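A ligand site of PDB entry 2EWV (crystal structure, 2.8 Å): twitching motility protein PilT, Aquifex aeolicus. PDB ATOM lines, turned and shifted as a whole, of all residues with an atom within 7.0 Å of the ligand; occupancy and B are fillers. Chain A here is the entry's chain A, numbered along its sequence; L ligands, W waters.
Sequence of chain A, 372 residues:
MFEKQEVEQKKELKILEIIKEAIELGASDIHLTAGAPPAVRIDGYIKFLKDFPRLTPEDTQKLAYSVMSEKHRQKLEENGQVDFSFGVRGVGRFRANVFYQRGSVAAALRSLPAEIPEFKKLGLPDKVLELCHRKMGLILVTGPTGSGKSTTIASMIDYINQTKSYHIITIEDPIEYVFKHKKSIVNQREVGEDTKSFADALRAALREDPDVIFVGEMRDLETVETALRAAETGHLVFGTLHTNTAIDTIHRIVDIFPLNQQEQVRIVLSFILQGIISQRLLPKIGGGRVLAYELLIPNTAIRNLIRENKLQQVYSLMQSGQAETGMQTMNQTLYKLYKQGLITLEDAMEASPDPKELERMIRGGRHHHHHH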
ATOM      1  N   PRO A 113     -27.184  30.594   7.553  1.00  0.00           N
ATOM      2  CA  PRO A 113     -27.156  30.856   6.112  1.00  0.00           C
ATOM      3  C   PRO A 113     -28.373  31.567   5.504  1.00  0.00           C
ATOM      4  O   PRO A 113     -29.487  31.044   5.495  1.00  0.00           O
ATOM      5  CB  PRO A 113     -26.941  29.461   5.522  1.00  0.00           C
ATOM      6  CG  PRO A 113     -26.223  28.729   6.605  1.00  0.00           C
ATOM      7  CD  PRO A 113     -27.009  29.158   7.821  1.00  0.00           C
ATOM      8  N   PRO A 117     -26.946  27.438  -1.678  1.00  0.00           N
ATOM      9  CA  PRO A 117     -25.999  27.119  -2.757  1.00  0.00           C
ATOM     10  C   PRO A 117     -26.590  26.442  -3.996  1.00  0.00           C
ATOM     11  O   PRO A 117     -27.475  25.604  -3.881  1.00  0.00           O
ATOM     12  CB  PRO A 117     -24.983  26.207  -2.065  1.00  0.00           C
ATOM     13  CG  PRO A 117     -25.038  26.633  -0.656  1.00  0.00           C
ATOM     14  CD  PRO A 117     -26.511  26.783  -0.422  1.00  0.00           C
ATOM     15  N   LYS A 121     -22.482  23.983  -7.499  1.00  0.00           N
ATOM     16  CA  LYS A 121     -21.376  24.358  -6.609  1.00  0.00           C
ATOM     17  C   LYS A 121     -21.045  23.296  -5.551  1.00  0.00           C
ATOM     18  O   LYS A 121     -19.908  23.225  -5.075  1.00  0.00           O
ATOM     19  CB  LYS A 121     -21.694  25.676  -5.893  1.00  0.00           C
ATOM     20  CG  LYS A 121     -22.115  26.820  -6.800  1.00  0.00           C
ATOM     21  CD  LYS A 121     -22.504  28.044  -5.972  1.00  0.00           C
ATOM     22  CE  LYS A 121     -23.165  29.113  -6.813  1.00  0.00           C
ATOM     23  NZ  LYS A 121     -23.946  30.087  -5.986  1.00  0.00           N
ATOM     24  N   LEU A 122     -22.043  22.513  -5.173  1.00  0.00           N
ATOM     25  CA  LEU A 122     -21.877  21.446  -4.191  1.00  0.00           C
ATOM     26  C   LEU A 122     -20.749  20.509  -4.617  1.00  0.00           C
ATOM     27  O   LEU A 122     -19.660  20.517  -4.032  1.00  0.00           O
ATOM     28  CB  LEU A 122     -23.182  20.661  -4.060  1.00  0.00           C
ATOM     29  CG  LEU A 122     -24.118  20.961  -2.875  1.00  0.00           C
ATOM     30  CD1 LEU A 122     -24.259  22.465  -2.645  1.00  0.00           C
ATOM     31  CD2 LEU A 122     -25.473  20.325  -3.154  1.00  0.00           C
ATOM     32  N   GLY A 123     -21.019  19.699  -5.635  1.00  0.00           N
ATOM     33  CA  GLY A 123     -20.023  18.770  -6.129  1.00  0.00           C
ATOM     34  C   GLY A 123     -20.654  17.473  -6.636  1.00  0.00           C
ATOM     35  O   GLY A 123     -20.097  16.830  -7.524  1.00  0.00           O
ATOM     36  N   LEU A 124     -21.816  17.107  -6.077  1.00  0.00           N
ATOM     37  CA  LEU A 124     -22.504  15.876  -6.478  1.00  0.00           C
ATOM     38  C   LEU A 124     -22.620  15.772  -7.984  1.00  0.00           C
ATOM     39  O   LEU A 124     -22.575  16.775  -8.686  1.00  0.00           O
ATOM     40  CB  LEU A 124     -23.903  15.811  -5.876  1.00  0.00           C
ATOM     41  CG  LEU A 124     -24.042  15.809  -4.371  1.00  0.00           C
ATOM     42  CD1 LEU A 124     -23.116  14.760  -3.770  1.00  0.00           C
ATOM     43  CD2 LEU A 124     -23.716  17.194  -3.826  1.00  0.00           C
ATOM     44  N   GLY A 143     -23.342  11.182   6.895  1.00  0.00           N
ATOM     45  CA  GLY A 143     -21.950  11.557   7.042  1.00  0.00           C
ATOM     46  C   GLY A 143     -21.612  12.096   8.412  1.00  0.00           C
ATOM     47  O   GLY A 143     -22.495  12.346   9.236  1.00  0.00           O
ATOM     48  N   PRO A 144     -20.324  12.277   8.689  1.00  0.00           N
ATOM     49  CA  PRO A 144     -19.950  12.809   9.994  1.00  0.00           C
ATOM     50  C   PRO A 144     -20.428  14.249  10.088  1.00  0.00           C
ATOM     51  O   PRO A 144     -20.426  14.977   9.080  1.00  0.00           O
ATOM     52  CB  PRO A 144     -18.426  12.698   9.988  1.00  0.00           C
ATOM     53  CG  PRO A 144     -18.094  12.954   8.540  1.00  0.00           C
ATOM     54  CD  PRO A 144     -19.130  12.115   7.826  1.00  0.00           C
ATOM     55  N   THR A 145     -20.853  14.671  11.269  1.00  0.00           N
ATOM     56  CA  THR A 145     -21.296  16.041  11.450  1.00  0.00           C
ATOM     57  C   THR A 145     -20.172  16.928  10.862  1.00  0.00           C
ATOM     58  O   THR A 145     -19.030  16.880  11.315  1.00  0.00           O
ATOM     59  CB  THR A 145     -21.544  16.370  12.951  1.00  0.00           C
ATOM     60  OG1 THR A 145     -21.367  15.176  13.740  1.00  0.00           O
ATOM     61  CG2 THR A 145     -22.976  16.883  13.155  1.00  0.00           C
ATOM     62  N   GLY A 146     -20.524  17.688   9.821  1.00  0.00           N
ATOM     63  CA  GLY A 146     -19.572  18.551   9.138  1.00  0.00           C
ATOM     64  C   GLY A 146     -19.190  17.997   7.774  1.00  0.00           C
ATOM     65  O   GLY A 146     -18.011  17.962   7.407  1.00  0.00           O
ATOM     66  N   SER A 147     -20.178  17.556   7.001  1.00  0.00           N
ATOM     67  CA  SER A 147     -19.891  16.986   5.693  1.00  0.00           C
ATOM     68  C   SER A 147     -20.834  17.410   4.563  1.00  0.00           C
ATOM     69  O   SER A 147     -20.923  16.717   3.548  1.00  0.00           O
ATOM     70  CB  SER A 147     -19.865  15.463   5.808  1.00  0.00           C
ATOM     71  OG  SER A 147     -21.025  14.997   6.463  1.00  0.00           O
ATOM     72  N   GLY A 148     -21.534  18.525   4.737  1.00  0.00           N
ATOM     73  CA  GLY A 148     -22.420  19.007   3.685  1.00  0.00           C
ATOM     74  C   GLY A 148     -23.848  18.529   3.658  1.00  0.00           C
ATOM     75  O   GLY A 148     -24.632  18.937   2.798  1.00  0.00           O
ATOM     76  N   LYS A 149     -24.208  17.669   4.600  1.00  0.00           N
ATOM     77  CA  LYS A 149     -25.557  17.125   4.673  1.00  0.00           C
ATOM     78  C   LYS A 149     -26.652  18.200   4.523  1.00  0.00           C
ATOM     79  O   LYS A 149     -27.460  18.132   3.607  1.00  0.00           O
ATOM     80  CB  LYS A 149     -25.753  16.352   5.995  1.00  0.00           C
ATOM     81  CG  LYS A 149     -24.787  15.177   6.231  1.00  0.00           C
ATOM     82  CD  LYS A 149     -25.210  14.315   7.437  1.00  0.00           C
ATOM     83  CE  LYS A 149     -24.987  15.009   8.773  1.00  0.00           C
ATOM     84  NZ  LYS A 149     -23.544  15.148   9.113  1.00  0.00           N
ATOM     85  N   SER A 150     -26.660  19.172   5.428  1.00  0.00           N
ATOM     86  CA  SER A 150     -27.646  20.266   5.407  1.00  0.00           C
ATOM     87  C   SER A 150     -27.727  20.902   4.040  1.00  0.00           C
ATOM     88  O   SER A 150     -28.800  20.998   3.440  1.00  0.00           O
ATOM     89  CB  SER A 150     -27.293  21.357   6.419  1.00  0.00           C
ATOM     90  OG  SER A 150     -27.517  20.955   7.763  1.00  0.00           O
ATOM     91  N   THR A 151     -26.573  21.364   3.562  1.00  0.00           N
ATOM     92  CA  THR A 151     -26.461  22.013   2.255  1.00  0.00           C
ATOM     93  C   THR A 151     -26.948  21.093   1.128  1.00  0.00           C
ATOM     94  O   THR A 151     -27.792  21.511   0.328  1.00  0.00           O
ATOM     95  CB  THR A 151     -24.996  22.472   1.977  1.00  0.00           C
ATOM     96  OG1 THR A 151     -24.476  23.144   3.132  1.00  0.00           O
ATOM     97  CG2 THR A 151     -24.949  23.428   0.795  1.00  0.00           C
ATOM     98  N   THR A 152     -26.418  19.866   1.055  1.00  0.00           N
ATOM     99  CA  THR A 152     -26.809  18.931   0.004  1.00  0.00           C
ATOM    100  C   THR A 152     -28.310  18.788  -0.022  1.00  0.00           C
ATOM    101  O   THR A 152     -28.899  18.713  -1.100  1.00  0.00           O
ATOM    102  CB  THR A 152     -26.234  17.510   0.196  1.00  0.00           C
ATOM    103  OG1 THR A 152     -24.824  17.519  -0.053  1.00  0.00           O
ATOM    104  CG2 THR A 152     -26.887  16.530  -0.772  1.00  0.00           C
ATOM    105  N   GLU A 176     -32.015  25.281   9.820  1.00  0.00           N
ATOM    106  CA  GLU A 176     -30.745  25.767   9.294  1.00  0.00           C
ATOM    107  C   GLU A 176     -31.024  26.737   8.138  1.00  0.00           C
ATOM    108  O   GLU A 176     -30.929  27.947   8.298  1.00  0.00           O
ATOM    109  CB  GLU A 176     -29.884  24.600   8.810  1.00  0.00           C
ATOM    110  CG  GLU A 176     -28.419  24.945   8.632  1.00  0.00           C
ATOM    111  CD  GLU A 176     -27.607  24.746   9.906  1.00  0.00           C
ATOM    112  OE1 GLU A 176     -26.435  25.194   9.909  1.00  0.00           O
ATOM    113  OE2 GLU A 176     -28.127  24.155  10.889  1.00  0.00           O
ATOM    114  N   TYR A 177     -31.341  26.188   6.964  1.00  0.00           N
ATOM    115  CA  TYR A 177     -31.657  27.033   5.819  1.00  0.00           C
ATOM    116  C   TYR A 177     -33.176  27.292   5.802  1.00  0.00           C
ATOM    117  O   TYR A 177     -33.971  26.478   6.279  1.00  0.00           O
ATOM    118  CB  TYR A 177     -31.251  26.388   4.486  1.00  0.00           C
ATOM    119  CG  TYR A 177     -29.754  26.310   4.203  1.00  0.00           C
ATOM    120  CD1 TYR A 177     -29.046  27.418   3.761  1.00  0.00           C
ATOM    121  CD2 TYR A 177     -29.063  25.101   4.336  1.00  0.00           C
ATOM    122  CE1 TYR A 177     -27.679  27.318   3.469  1.00  0.00           C
ATOM    123  CE2 TYR A 177     -27.707  24.991   4.057  1.00  0.00           C
ATOM    124  CZ  TYR A 177     -27.016  26.102   3.617  1.00  0.00           C
ATOM    125  OH  TYR A 177     -25.674  25.969   3.354  1.00  0.00           O
ATOM    126  N   HIS A 242     -26.009   9.490  10.588  1.00  0.00           N
ATOM    127  CA  HIS A 242     -24.621   9.892  10.751  1.00  0.00           C
ATOM    128  C   HIS A 242     -23.593   8.850  10.296  1.00  0.00           C
ATOM    129  O   HIS A 242     -22.407   8.980  10.582  1.00  0.00           O
ATOM    130  CB  HIS A 242     -24.346  10.303  12.214  1.00  0.00           C
ATOM    131  CG  HIS A 242     -24.538  11.762  12.472  1.00  0.00           C
ATOM    132  ND1 HIS A 242     -24.257  12.337  13.694  1.00  0.00           N
ATOM    133  CD2 HIS A 242     -24.966  12.774  11.675  1.00  0.00           C
ATOM    134  CE1 HIS A 242     -24.496  13.638  13.637  1.00  0.00           C
ATOM    135  NE2 HIS A 242     -24.924  13.926  12.421  1.00  0.00           N
ATOM    136  N   GLN A 279     -21.201  11.377   2.716  1.00  0.00           N
ATOM    137  CA  GLN A 279     -20.225  12.426   2.440  1.00  0.00           C
ATOM    138  C   GLN A 279     -19.177  12.617   3.526  1.00  0.00           C
ATOM    139  O   GLN A 279     -19.386  12.283   4.689  1.00  0.00           O
ATOM    140  CB  GLN A 279     -20.945  13.759   2.206  1.00  0.00           C
ATOM    141  CG  GLN A 279     -22.015  13.755   1.117  1.00  0.00           C
ATOM    142  CD  GLN A 279     -22.807  15.063   1.030  1.00  0.00           C
ATOM    143  OE1 GLN A 279     -23.664  15.221   0.163  1.00  0.00           O
ATOM    144  NE2 GLN A 279     -22.514  16.006   1.923  1.00  0.00           N
ATOM    145  N   LEU A 281     -16.061  15.808   4.038  1.00  0.00           N
ATOM    146  CA  LEU A 281     -15.467  16.979   3.417  1.00  0.00           C
ATOM    147  C   LEU A 281     -13.947  17.052   3.546  1.00  0.00           C
ATOM    148  O   LEU A 281     -13.428  17.531   4.556  1.00  0.00           O
ATOM    149  CB  LEU A 281     -16.087  18.258   3.972  1.00  0.00           C
ATOM    150  CG  LEU A 281     -17.520  18.486   3.545  1.00  0.00           C
ATOM    151  CD1 LEU A 281     -17.904  19.937   3.841  1.00  0.00           C
ATOM    152  CD2 LEU A 281     -17.666  18.186   2.066  1.00  0.00           C
ATOM    153  N   ARG A 289     -12.005  23.178   0.459  1.00  0.00           N
ATOM    154  CA  ARG A 289     -13.127  22.258   0.424  1.00  0.00           C
ATOM    155  C   ARG A 289     -13.440  21.560  -0.920  1.00  0.00           C
ATOM    156  O   ARG A 289     -13.542  22.195  -1.968  1.00  0.00           O
ATOM    157  CB  ARG A 289     -14.347  23.009   0.967  1.00  0.00           C
ATOM    158  CG  ARG A 289     -14.084  24.492   1.235  1.00  0.00           C
ATOM    159  CD  ARG A 289     -14.409  25.279   0.008  1.00  0.00           C
ATOM    160  NE  ARG A 289     -15.392  26.261   0.398  1.00  0.00           N
ATOM    161  CZ  ARG A 289     -16.502  26.517  -0.286  1.00  0.00           C
ATOM    162  NH1 ARG A 289     -16.777  25.865  -1.405  1.00  0.00           N
ATOM    163  NH2 ARG A 289     -17.338  27.421   0.193  1.00  0.00           N
ATOM    164  N   VAL A 290     -13.523  20.232  -0.849  1.00  0.00           N
ATOM    165  CA  VAL A 290     -13.844  19.338  -1.961  1.00  0.00           C
ATOM    166  C   VAL A 290     -14.575  18.223  -1.253  1.00  0.00           C
ATOM    167  O   VAL A 290     -14.437  18.046  -0.046  1.00  0.00           O
ATOM    168  CB  VAL A 290     -12.591  18.716  -2.640  1.00  0.00           C
ATOM    169  CG1 VAL A 290     -13.010  17.727  -3.741  1.00  0.00           C
ATOM    170  CG2 VAL A 290     -11.746  19.810  -3.231  1.00  0.00           C
ATOM    171  N   LEU A 291     -15.330  17.433  -2.000  1.00  0.00           N
ATOM    172  CA  LEU A 291     -16.090  16.418  -1.319  1.00  0.00           C
ATOM    173  C   LEU A 291     -15.953  14.978  -1.781  1.00  0.00           C
ATOM    174  O   LEU A 291     -16.038  14.689  -2.967  1.00  0.00           O
ATOM    175  CB  LEU A 291     -17.541  16.858  -1.371  1.00  0.00           C
ATOM    176  CG  LEU A 291     -18.735  15.924  -1.190  1.00  0.00           C
ATOM    177  CD1 LEU A 291     -19.041  15.657   0.290  1.00  0.00           C
ATOM    178  CD2 LEU A 291     -19.919  16.604  -1.869  1.00  0.00           C
HETATM  179  P1  LIG L   1     -23.669  19.309   8.299  1.00  0.00           P
HETATM  180  O1  LIG L   1     -23.593  18.853   9.704  1.00  0.00           O
HETATM  181  O2  LIG L   1     -23.060  18.161   7.340  1.00  0.00           O
HETATM  182  O3  LIG L   1     -25.210  19.561   7.963  1.00  0.00           O
HETATM  183  P2  LIG L   1     -23.252  21.563   6.775  1.00  0.00           P
HETATM  184  O4  LIG L   1     -24.032  20.764   5.813  1.00  0.00           O
HETATM  185  O5  LIG L   1     -24.110  22.865   7.240  1.00  0.00           O
HETATM  186  O6  LIG L   1     -22.828  20.703   8.113  1.00  0.00           O
HETATM  187  O7  LIG L   1     -21.909  22.063   6.032  1.00  0.00           O
HETATM  188  C1  LIG L   1     -21.173  22.932   6.930  1.00  0.00           C
HETATM  189  C2  LIG L   1     -20.212  23.852   6.159  1.00  0.00           C
HETATM  190  O8  LIG L   1     -19.599  23.143   5.025  1.00  0.00           O
HETATM  191  C3  LIG L   1     -20.961  25.074   5.599  1.00  0.00           C
HETATM  192  O9  LIG L   1     -20.200  26.261   5.819  1.00  0.00           O
HETATM  193  C4  LIG L   1     -21.128  24.736   4.103  1.00  0.00           C
HETATM  194  O10 LIG L   1     -21.204  25.902   3.260  1.00  0.00           O
HETATM  195  C5  LIG L   1     -19.933  23.831   3.777  1.00  0.00           C
HETATM  196  N1  LIG L   1     -20.297  22.836   2.735  1.00  0.00           N
HETATM  197  C6  LIG L   1     -21.398  22.004   2.738  1.00  0.00           C
HETATM  198  N2  LIG L   1     -21.428  21.253   1.671  1.00  0.00           N
HETATM  199  C7  LIG L   1     -20.350  21.550   0.893  1.00  0.00           C
HETATM  200  C8  LIG L   1     -19.862  21.077  -0.361  1.00  0.00           C
HETATM  201  N3  LIG L   1     -20.537  20.089  -1.062  1.00  0.00           N
HETATM  202  N4  LIG L   1     -18.709  21.615  -0.861  1.00  0.00           N
HETATM  203  C9  LIG L   1     -18.039  22.565  -0.193  1.00  0.00           C
HETATM  204  N5  LIG L   1     -18.471  23.041   0.990  1.00  0.00           N
HETATM  205  C10 LIG L   1     -19.606  22.579   1.563  1.00  0.00           C
HETATM  206  O   HOH W   1     -23.442  27.078   4.883  1.00  0.00           O
HETATM  207  O   HOH W   2     -26.201  20.819  10.031  1.00  0.00           O
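The side-chain hydroxyl (OG) of Ser 147 lies within hydrogen-bond range of the backbone carbonyl oxygen (O) of Pro 144 (2.7 Å). The side-chain amino group (NZ) of Lys 149 is in hydrogen-bond range of the backbone carbonyl oxygen (O) of Pro 144, 3.1 Å away. The backbone carbonyl oxygen (O) of Gly 148 sits at hydrogen-bond distance from the side-chain hydroxyl (OG1) of Thr 152. NZ of Lys 149 is in hydrogen-bond range of O of Gly 143. OG1 of Thr 151 lies within hydrogen-bond range of OH of Tyr 177.
Merely in contact with the ligand: Leu 291, Arg 289 and Leu 281. Hydrophobic or aromatic side chains within 4 Å of the ligand: Leu 281 and Leu 291. The nearest printed residue that does not touch the ligand is Thr 145 (4.02 Å).
Water W2 lies within hydrogen-bond range of an oxygen (O3) of the ligand (2.6 Å) and the side-chain hydroxyl of Ser 150 (2.6 Å). Water W1 bridges the side-chain hydroxyl (OH) of Tyr 177 (2.9 Å) and an oxygen (O10) of the ligand (3.0 Å).
The backbone NH (N) of Gly 146 lies within hydrogen-bond range of an oxygen (O1) of the ligand. OG of Ser 150 lies within hydrogen-bond range of O3 of the ligand, at 2.7 Å. An oxygen (O3) of the ligand lies within hydrogen-bond range of the backbone NH (N) of Ser 150, 2.9 Å away. The backbone NH of Lys 149 sits at hydrogen-bond distance from an oxygen (O2) of the ligand, at 3.0 Å. O2 of the ligand sits at hydrogen-bond distance from N of Gly 148, 3.0 Å away. NZ of Lys 149 is in salt-bridge range of O2 of the ligand (3.5 Å). The backbone carbonyl oxygen of Leu 122 sits at hydrogen-bond distance from a nitrogen (N3) of the ligand (3.1 Å). The backbone NH of Ser 147 sits at hydrogen-bond distance from an oxygen (O2) of the ligand, 3.0 Å away. An oxygen (O4) of the ligand lies within hydrogen-bond range of the backbone NH of Thr 151 (3.4 Å).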
